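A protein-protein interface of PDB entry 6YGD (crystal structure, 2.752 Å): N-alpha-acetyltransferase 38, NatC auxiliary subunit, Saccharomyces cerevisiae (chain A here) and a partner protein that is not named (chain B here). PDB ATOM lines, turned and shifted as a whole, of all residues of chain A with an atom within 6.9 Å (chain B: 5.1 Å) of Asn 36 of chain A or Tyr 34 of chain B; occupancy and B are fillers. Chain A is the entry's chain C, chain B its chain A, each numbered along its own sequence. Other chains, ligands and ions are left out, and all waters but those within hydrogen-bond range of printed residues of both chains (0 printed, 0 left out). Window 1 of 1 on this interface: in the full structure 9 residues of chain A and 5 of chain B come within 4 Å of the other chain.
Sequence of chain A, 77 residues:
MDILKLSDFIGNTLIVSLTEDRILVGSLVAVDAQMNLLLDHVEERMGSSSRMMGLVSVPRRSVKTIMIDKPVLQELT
The side-chain hydroxyl (OH) of Tyr 34 of chain B is in hydrogen-bond range of the backbone carbonyl oxygen (O) of Ala 30 of chain A (3.2 Å). The side-chain hydroxyl of Tyr 34 of chain B sits at hydrogen-bond distance from the backbone NH of Val 31 of chain A, at 3.5 Å. The backbone carbonyl oxygen of Asn 36 of chain A sits at hydrogen-bond distance from the side-chain hydroxyl of Tyr 34 of chain B. The guanidinium group of Arg 37 of chain B lies within salt-bridge range of the side-chain carboxylate of Asp 32 of chain A (3.3 Å).
Printed residues of chain B within 4 Å of Asn 36 of chain A: Ile 33 and Tyr 34. Tyr 34 of chain B touches just these residues of chain A: Ala 30, Val 31, Asp 32, Asn 36, Leu 37, Leu 38 and Ser 57. Printed residues of chain B within 4 Å of Leu 37 of chain A: Tyr 34. Of the printed residues of chain B, Val 31 of chain A touches Tyr 34 (3.5 Å). Tyr 38 of chain B touches none of the printed residues of chain A. The nearest printed residue of chain B that does not touch Asp 32 of chain A is Ile 33 of chain B (4.3 Å).
The side-chain hydroxyl of Ser 32 of chain B lies close to the backbone NH of Tyr 34 of chain B, 3.4 Å away. The backbone NH of Val 29 of chain A is in hydrogen-bond range of the backbone carbonyl oxygen of Leu 38 of chain A. O of Ala 30 of chain A lies within hydrogen-bond range of N of Leu 38 of chain A, at 3.0 Å. N of Gln 34 of chain A lies close to OD1 of Asp 32 of chain A, at 3.3 Å. N of Met 35 of chain A lies within hydrogen-bond range of OD1 of Asp 32 of chain A (3.1 Å). The side-chain amide oxygen of Asn 36 of chain A sits at hydrogen-bond distance from the backbone NH of Arg 60 of chain A (2.8 Å).
OH of Tyr 34 of chain B touches N of Asp 32 of chain A (3.8 Å). Ile 33 of chain B touches Asn 36 of chain A (CD1 to ND2, 3.8 Å). Tyr 34 of chain B touches Leu 37 of chain A (CE1 to O, 3.9 Å). Leu 38 of chain A touches Tyr 34 of chain B (CB to CZ, 3.5 Å). Ser 32 of chain B touches Ser 57 of chain A. CD1 of Tyr 34 of chain B touches CB of Ser 57 of chain A, at 3.6 Å. CD1 of Ile 33 of chain B touches CG of Pro 59 of chain A, at 3.8 Å.
Of the 19 printed residues of chain A, 8 touch a printed residue of chain B. Hydrophobic or aromatic side chains of chain A within 4 Å of the printed part of chain B: Ala 30, Leu 38 and Pro 59. Among the printed residues, Asp or Glu carboxylates within 4 Å of a Lys or Arg side-chain nitrogen of the other chain: Asp 32 of chain A with Arg 37 of chain B (3.3 Å).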
ATOM      1  N   LEU A  28     -14.621   8.640   6.951  1.00  0.00           N
ATOM      2  CA  LEU A  28     -13.228   8.303   7.210  1.00  0.00           C
ATOM      3  C   LEU A  28     -13.129   7.000   7.989  1.00  0.00           C
ATOM      4  O   LEU A  28     -13.614   6.905   9.121  1.00  0.00           O
ATOM      5  CB  LEU A  28     -12.556   9.433   7.982  1.00  0.00           C
ATOM      6  CG  LEU A  28     -11.044   9.333   8.177  1.00  0.00           C
ATOM      7  CD1 LEU A  28     -10.321   9.476   6.843  1.00  0.00           C
ATOM      8  CD2 LEU A  28     -10.564  10.379   9.171  1.00  0.00           C
ATOM      9  N   VAL A  29     -12.500   5.996   7.385  1.00  0.00           N
ATOM     10  CA  VAL A  29     -12.296   4.719   8.061  1.00  0.00           C
ATOM     11  C   VAL A  29     -10.971   4.698   8.810  1.00  0.00           C
ATOM     12  O   VAL A  29     -10.906   4.225   9.948  1.00  0.00           O
ATOM     13  CB  VAL A  29     -12.379   3.557   7.050  1.00  0.00           C
ATOM     14  CG1 VAL A  29     -12.391   2.223   7.778  1.00  0.00           C
ATOM     15  CG2 VAL A  29     -13.605   3.697   6.181  1.00  0.00           C
ATOM     16  N   ALA A  30      -9.908   5.213   8.191  1.00  0.00           N
ATOM     17  CA  ALA A  30      -8.583   5.176   8.795  1.00  0.00           C
ATOM     18  C   ALA A  30      -7.714   6.278   8.203  1.00  0.00           C
ATOM     19  O   ALA A  30      -8.013   6.833   7.142  1.00  0.00           O
ATOM     20  CB  ALA A  30      -7.919   3.808   8.603  1.00  0.00           C
ATOM     21  N   VAL A  31      -6.628   6.579   8.911  1.00  0.00           N
ATOM     22  CA  VAL A  31      -5.650   7.589   8.507  1.00  0.00           C
ATOM     23  C   VAL A  31      -4.272   7.094   8.928  1.00  0.00           C
ATOM     24  O   VAL A  31      -4.101   6.599  10.045  1.00  0.00           O
ATOM     25  CB  VAL A  31      -5.970   8.963   9.143  1.00  0.00           C
ATOM     26  CG1 VAL A  31      -4.749   9.869   9.142  1.00  0.00           C
ATOM     27  CG2 VAL A  31      -7.121   9.639   8.426  1.00  0.00           C
ATOM     28  N   ASP A  32      -3.289   7.213   8.037  1.00  0.00           N
ATOM     29  CA  ASP A  32      -1.918   6.831   8.354  1.00  0.00           C
ATOM     30  C   ASP A  32      -1.058   8.066   8.606  1.00  0.00           C
ATOM     31  O   ASP A  32      -1.507   9.209   8.480  1.00  0.00           O
ATOM     32  CB  ASP A  32      -1.310   5.961   7.242  1.00  0.00           C
ATOM     33  CG  ASP A  32      -1.143   6.703   5.927  1.00  0.00           C
ATOM     34  OD1 ASP A  32      -1.489   7.898   5.847  1.00  0.00           O
ATOM     35  OD2 ASP A  32      -0.662   6.079   4.960  1.00  0.00           O
ATOM     36  N   ALA A  33       0.209   7.813   8.952  1.00  0.00           N
ATOM     37  CA  ALA A  33       1.130   8.882   9.321  1.00  0.00           C
ATOM     38  C   ALA A  33       1.392   9.857   8.181  1.00  0.00           C
ATOM     39  O   ALA A  33       1.745  11.013   8.438  1.00  0.00           O
ATOM     40  CB  ALA A  33       2.450   8.289   9.795  1.00  0.00           C
ATOM     41  N   GLN A  34       1.228   9.423   6.935  1.00  0.00           N
ATOM     42  CA  GLN A  34       1.411  10.300   5.789  1.00  0.00           C
ATOM     43  C   GLN A  34       0.112  10.966   5.355  1.00  0.00           C
ATOM     44  O   GLN A  34       0.046  11.508   4.246  1.00  0.00           O
ATOM     45  CB  GLN A  34       2.018   9.522   4.617  1.00  0.00           C
ATOM     46  CG  GLN A  34       3.193   8.623   4.982  1.00  0.00           C
ATOM     47  CD  GLN A  34       4.287   9.366   5.713  1.00  0.00           C
ATOM     48  OE1 GLN A  34       4.579  10.520   5.402  1.00  0.00           O
ATOM     49  NE2 GLN A  34       4.888   8.716   6.702  1.00  0.00           N
ATOM     50  N   MET A  35      -0.916  10.923   6.206  1.00  0.00           N
ATOM     51  CA  MET A  35      -2.237  11.503   5.970  1.00  0.00           C
ATOM     52  C   MET A  35      -2.955  10.884   4.770  1.00  0.00           C
ATOM     53  O   MET A  35      -3.845  11.511   4.185  1.00  0.00           O
ATOM     54  CB  MET A  35      -2.157  13.030   5.825  1.00  0.00           C
ATOM     55  CG  MET A  35      -3.446  13.772   6.161  1.00  0.00           C
ATOM     56  SD  MET A  35      -3.355  15.508   5.698  1.00  0.00           S
ATOM     57  CE  MET A  35      -3.134  15.346   3.928  1.00  0.00           C
ATOM     58  N   ASN A  36      -2.592   9.662   4.387  1.00  0.00           N
ATOM     59  CA  ASN A  36      -3.388   8.913   3.423  1.00  0.00           C
ATOM     60  C   ASN A  36      -4.700   8.486   4.070  1.00  0.00           C
ATOM     61  O   ASN A  36      -4.712   7.933   5.174  1.00  0.00           O
ATOM     62  CB  ASN A  36      -2.625   7.685   2.922  1.00  0.00           C
ATOM     63  CG  ASN A  36      -1.340   8.044   2.197  1.00  0.00           C
ATOM     64  OD1 ASN A  36      -1.294   9.008   1.436  1.00  0.00           O
ATOM     65  ND2 ASN A  36      -0.288   7.266   2.432  1.00  0.00           N
ATOM     66  N   LEU A  37      -5.811   8.744   3.381  1.00  0.00           N
ATOM     67  CA  LEU A  37      -7.139   8.543   3.942  1.00  0.00           C
ATOM     68  C   LEU A  37      -7.785   7.285   3.378  1.00  0.00           C
ATOM     69  O   LEU A  37      -7.599   6.951   2.204  1.00  0.00           O
ATOM     70  CB  LEU A  37      -8.036   9.753   3.662  1.00  0.00           C
ATOM     71  CG  LEU A  37      -7.399  11.130   3.849  1.00  0.00           C
ATOM     72  CD1 LEU A  37      -8.344  12.209   3.358  1.00  0.00           C
ATOM     73  CD2 LEU A  37      -7.017  11.372   5.299  1.00  0.00           C
ATOM     74  N   LEU A  38      -8.541   6.589   4.225  1.00  0.00           N
ATOM     75  CA  LEU A  38      -9.383   5.472   3.814  1.00  0.00           C
ATOM     76  C   LEU A  38     -10.826   5.844   4.123  1.00  0.00           C
ATOM     77  O   LEU A  38     -11.173   6.076   5.286  1.00  0.00           O
ATOM     78  CB  LEU A  38      -8.990   4.182   4.532  1.00  0.00           C
ATOM     79  CG  LEU A  38      -9.814   2.927   4.221  1.00  0.00           C
ATOM     80  CD1 LEU A  38      -9.572   2.440   2.797  1.00  0.00           C
ATOM     81  CD2 LEU A  38      -9.513   1.819   5.227  1.00  0.00           C
ATOM     82  N   LEU A  39     -11.657   5.917   3.085  1.00  0.00           N
ATOM     83  CA  LEU A  39     -13.037   6.362   3.212  1.00  0.00           C
ATOM     84  C   LEU A  39     -13.976   5.274   2.712  1.00  0.00           C
ATOM     85  O   LEU A  39     -13.733   4.668   1.665  1.00  0.00           O
ATOM     86  CB  LEU A  39     -13.274   7.657   2.422  1.00  0.00           C
ATOM     87  CG  LEU A  39     -12.288   8.817   2.586  1.00  0.00           C
ATOM     88  CD1 LEU A  39     -12.453   9.816   1.452  1.00  0.00           C
ATOM     89  CD2 LEU A  39     -12.472   9.508   3.923  1.00  0.00           C
ATOM     90  N   VAL A  56     -12.663   3.590  -0.707  1.00  0.00           N
ATOM     91  CA  VAL A  56     -11.612   4.213  -1.502  1.00  0.00           C
ATOM     92  C   VAL A  56     -10.526   4.736  -0.571  1.00  0.00           C
ATOM     93  O   VAL A  56     -10.817   5.243   0.519  1.00  0.00           O
ATOM     94  CB  VAL A  56     -12.167   5.356  -2.381  1.00  0.00           C
ATOM     95  CG1 VAL A  56     -11.098   5.866  -3.337  1.00  0.00           C
ATOM     96  CG2 VAL A  56     -13.399   4.900  -3.148  1.00  0.00           C
ATOM     97  N   SER A  57      -9.273   4.608  -0.997  1.00  0.00           N
ATOM     98  CA  SER A  57      -8.139   5.204  -0.305  1.00  0.00           C
ATOM     99  C   SER A  57      -7.552   6.299  -1.184  1.00  0.00           C
ATOM    100  O   SER A  57      -7.347   6.086  -2.384  1.00  0.00           O
ATOM    101  CB  SER A  57      -7.072   4.156   0.015  1.00  0.00           C
ATOM    102  OG  SER A  57      -6.322   3.835  -1.145  1.00  0.00           O
ATOM    103  N   VAL A  58      -7.283   7.459  -0.596  1.00  0.00           N
ATOM    104  CA  VAL A  58      -6.781   8.613  -1.331  1.00  0.00           C
ATOM    105  C   VAL A  58      -5.380   8.950  -0.830  1.00  0.00           C
ATOM    106  O   VAL A  58      -5.172   9.124   0.374  1.00  0.00           O
ATOM    107  CB  VAL A  58      -7.719   9.828  -1.228  1.00  0.00           C
ATOM    108  CG1 VAL A  58      -9.100   9.451  -1.743  1.00  0.00           C
ATOM    109  CG2 VAL A  58      -7.819  10.360   0.198  1.00  0.00           C
ATOM    110  N   PRO A  59      -4.381   9.003  -1.704  1.00  0.00           N
ATOM    111  CA  PRO A  59      -3.041   9.409  -1.277  1.00  0.00           C
ATOM    112  C   PRO A  59      -3.010  10.883  -0.904  1.00  0.00           C
ATOM    113  O   PRO A  59      -3.887  11.664  -1.274  1.00  0.00           O
ATOM    114  CB  PRO A  59      -2.176   9.125  -2.509  1.00  0.00           C
ATOM    115  CG  PRO A  59      -2.959   8.103  -3.288  1.00  0.00           C
ATOM    116  CD  PRO A  59      -4.389   8.473  -3.076  1.00  0.00           C
ATOM    117  N   ARG A  60      -1.975  11.252  -0.143  1.00  0.00           N
ATOM    118  CA  ARG A  60      -1.826  12.639   0.287  1.00  0.00           C
ATOM    119  C   ARG A  60      -1.735  13.590  -0.903  1.00  0.00           C
ATOM    120  O   ARG A  60      -2.354  14.661  -0.901  1.00  0.00           O
ATOM    121  CB  ARG A  60      -0.591  12.779   1.178  1.00  0.00           C
ATOM    122  CG  ARG A  60      -0.167  14.214   1.437  1.00  0.00           C
ATOM    123  CD  ARG A  60       1.155  14.286   2.181  1.00  0.00           C
ATOM    124  NE  ARG A  60       1.699  15.642   2.174  1.00  0.00           N
ATOM    125  CZ  ARG A  60       1.400  16.575   3.073  1.00  0.00           C
ATOM    126  NH1 ARG A  60       0.556  16.301   4.060  1.00  0.00           N
ATOM    127  NH2 ARG A  60       1.943  17.783   2.986  1.00  0.00           N
ATOM    128  N   ARG A  61      -0.971  13.211  -1.931  1.00  0.00           N
ATOM    129  CA  ARG A  61      -0.774  14.085  -3.084  1.00  0.00           C
ATOM    130  C   ARG A  61      -2.060  14.313  -3.867  1.00  0.00           C
ATOM    131  O   ARG A  61      -2.165  15.307  -4.594  1.00  0.00           O
ATOM    132  CB  ARG A  61       0.305  13.503  -3.999  1.00  0.00           C
ATOM    133  CG  ARG A  61       1.665  13.347  -3.329  1.00  0.00           C
ATOM    134  CD  ARG A  61       2.642  12.581  -4.210  1.00  0.00           C
ATOM    135  NE  ARG A  61       3.940  12.392  -3.564  1.00  0.00           N
ATOM    136  CZ  ARG A  61       4.976  13.214  -3.708  1.00  0.00           C
ATOM    137  NH1 ARG A  61       4.869  14.289  -4.478  1.00  0.00           N
ATOM    138  NH2 ARG A  61       6.119  12.964  -3.084  1.00  0.00           N
ATOM    139  N   VAL A  63      -5.028  14.747  -2.396  1.00  0.00           N
ATOM    140  CA  VAL A  63      -5.924  15.565  -1.586  1.00  0.00           C
ATOM    141  C   VAL A  63      -5.574  17.038  -1.771  1.00  0.00           C
ATOM    142  O   VAL A  63      -4.452  17.465  -1.479  1.00  0.00           O
ATOM    143  CB  VAL A  63      -5.853  15.165  -0.107  1.00  0.00           C
ATOM    144  CG1 VAL A  63      -6.545  16.207   0.745  1.00  0.00           C
ATOM    145  CG2 VAL A  63      -6.487  13.799   0.100  1.00  0.00           C
ATOM    146  N   SER B  32      -3.761  -1.094  -3.559  1.00  0.00           N
ATOM    147  CA  SER B  32      -3.796   0.269  -3.049  1.00  0.00           C
ATOM    148  C   SER B  32      -2.779   0.424  -1.920  1.00  0.00           C
ATOM    149  O   SER B  32      -2.113  -0.530  -1.511  1.00  0.00           O
ATOM    150  CB  SER B  32      -5.202   0.644  -2.577  1.00  0.00           C
ATOM    151  OG  SER B  32      -5.548   0.003  -1.359  1.00  0.00           O
ATOM    152  N   ILE B  33      -2.655   1.655  -1.416  1.00  0.00           N
ATOM    153  CA  ILE B  33      -1.739   1.925  -0.311  1.00  0.00           C
ATOM    154  C   ILE B  33      -2.086   1.065   0.897  1.00  0.00           C
ATOM    155  O   ILE B  33      -1.193   0.566   1.595  1.00  0.00           O
ATOM    156  CB  ILE B  33      -1.756   3.434   0.026  1.00  0.00           C
ATOM    157  CG1 ILE B  33      -0.832   4.204  -0.925  1.00  0.00           C
ATOM    158  CG2 ILE B  33      -1.376   3.689   1.478  1.00  0.00           C
ATOM    159  CD1 ILE B  33      -1.098   5.702  -0.961  1.00  0.00           C
ATOM    160  N   TYR B  34      -3.382   0.837   1.137  1.00  0.00           N
ATOM    161  CA  TYR B  34      -3.809   0.126   2.335  1.00  0.00           C
ATOM    162  C   TYR B  34      -3.618  -1.380   2.238  1.00  0.00           C
ATOM    163  O   TYR B  34      -3.683  -2.062   3.266  1.00  0.00           O
ATOM    164  CB  TYR B  34      -5.264   0.470   2.659  1.00  0.00           C
ATOM    165  CG  TYR B  34      -5.366   1.693   3.542  1.00  0.00           C
ATOM    166  CD1 TYR B  34      -5.352   2.969   3.000  1.00  0.00           C
ATOM    167  CD2 TYR B  34      -5.444   1.569   4.924  1.00  0.00           C
ATOM    168  CE1 TYR B  34      -5.429   4.085   3.808  1.00  0.00           C
ATOM    169  CE2 TYR B  34      -5.523   2.680   5.737  1.00  0.00           C
ATOM    170  CZ  TYR B  34      -5.514   3.933   5.173  1.00  0.00           C
ATOM    171  OH  TYR B  34      -5.593   5.042   5.976  1.00  0.00           O
ATOM    172  N   VAL B  35      -3.378  -1.915   1.041  1.00  0.00           N
ATOM    173  CA  VAL B  35      -2.922  -3.297   0.942  1.00  0.00           C
ATOM    174  C   VAL B  35      -1.527  -3.419   1.540  1.00  0.00           C
ATOM    175  O   VAL B  35      -1.275  -4.254   2.417  1.00  0.00           O
ATOM    176  CB  VAL B  35      -2.958  -3.780  -0.519  1.00  0.00           C
ATOM    177  CG1 VAL B  35      -2.476  -5.214  -0.607  1.00  0.00           C
ATOM    178  CG2 VAL B  35      -4.358  -3.649  -1.093  1.00  0.00           C
ATOM    179  N   TYR B  36      -0.605  -2.560   1.088  1.00  0.00           N
ATOM    180  CA  TYR B  36       0.734  -2.526   1.668  1.00  0.00           C
ATOM    181  C   TYR B  36       0.684  -2.113   3.131  1.00  0.00           C
ATOM    182  O   TYR B  36       1.466  -2.605   3.952  1.00  0.00           O
ATOM    183  CB  TYR B  36       1.631  -1.564   0.885  1.00  0.00           C
ATOM    184  CG  TYR B  36       1.728  -1.841  -0.597  1.00  0.00           C
ATOM    185  CD1 TYR B  36       2.569  -2.832  -1.088  1.00  0.00           C
ATOM    186  CD2 TYR B  36       0.997  -1.096  -1.509  1.00  0.00           C
ATOM    187  CE1 TYR B  36       2.665  -3.083  -2.444  1.00  0.00           C
ATOM    188  CE2 TYR B  36       1.085  -1.340  -2.865  1.00  0.00           C
ATOM    189  CZ  TYR B  36       1.922  -2.335  -3.329  1.00  0.00           C
ATOM    190  OH  TYR B  36       2.011  -2.578  -4.682  1.00  0.00           O
ATOM    191  N   ARG B  37      -0.229  -1.203   3.476  1.00  0.00           N
ATOM    192  CA  ARG B  37      -0.334  -0.753   4.860  1.00  0.00           C
ATOM    193  C   ARG B  37      -0.780  -1.880   5.780  1.00  0.00           C
ATOM    194  O   ARG B  37      -0.355  -1.941   6.939  1.00  0.00           O
ATOM    195  CB  ARG B  37      -1.299   0.431   4.954  1.00  0.00           C
ATOM    196  CG  ARG B  37      -0.868   1.503   5.934  1.00  0.00           C
ATOM    197  CD  ARG B  37       0.321   2.292   5.410  1.00  0.00           C
ATOM    198  NE  ARG B  37       1.022   2.984   6.487  1.00  0.00           N
ATOM    199  CZ  ARG B  37       1.890   3.975   6.310  1.00  0.00           C
ATOM    200  NH1 ARG B  37       2.166   4.412   5.088  1.00  0.00           N
ATOM    201  NH2 ARG B  37       2.476   4.538   7.357  1.00  0.00           N
ATOM    202  N   TYR B  38      -1.627  -2.786   5.284  1.00  0.00           N
ATOM    203  CA  TYR B  38      -2.058  -3.924   6.091  1.00  0.00           C
ATOM    204  C   TYR B  38      -0.900  -4.872   6.375  1.00  0.00           C
ATOM    205  O   TYR B  38      -0.785  -5.405   7.485  1.00  0.00           O
ATOM    206  CB  TYR B  38      -3.204  -4.652   5.385  1.00  0.00           C
ATOM    207  CG  TYR B  38      -3.383  -6.108   5.768  1.00  0.00           C
ATOM    208  CD1 TYR B  38      -4.053  -6.467   6.932  1.00  0.00           C
ATOM    209  CD2 TYR B  38      -2.902  -7.123   4.949  1.00  0.00           C
ATOM    210  CE1 TYR B  38      -4.227  -7.797   7.277  1.00  0.00           C
ATOM    211  CE2 TYR B  38      -3.068  -8.455   5.285  1.00  0.00           C
ATOM    212  CZ  TYR B  38      -3.733  -8.787   6.448  1.00  0.00           C
ATOM    213  OH  TYR B  38      -3.899 -10.114   6.778  1.00  0.00           O
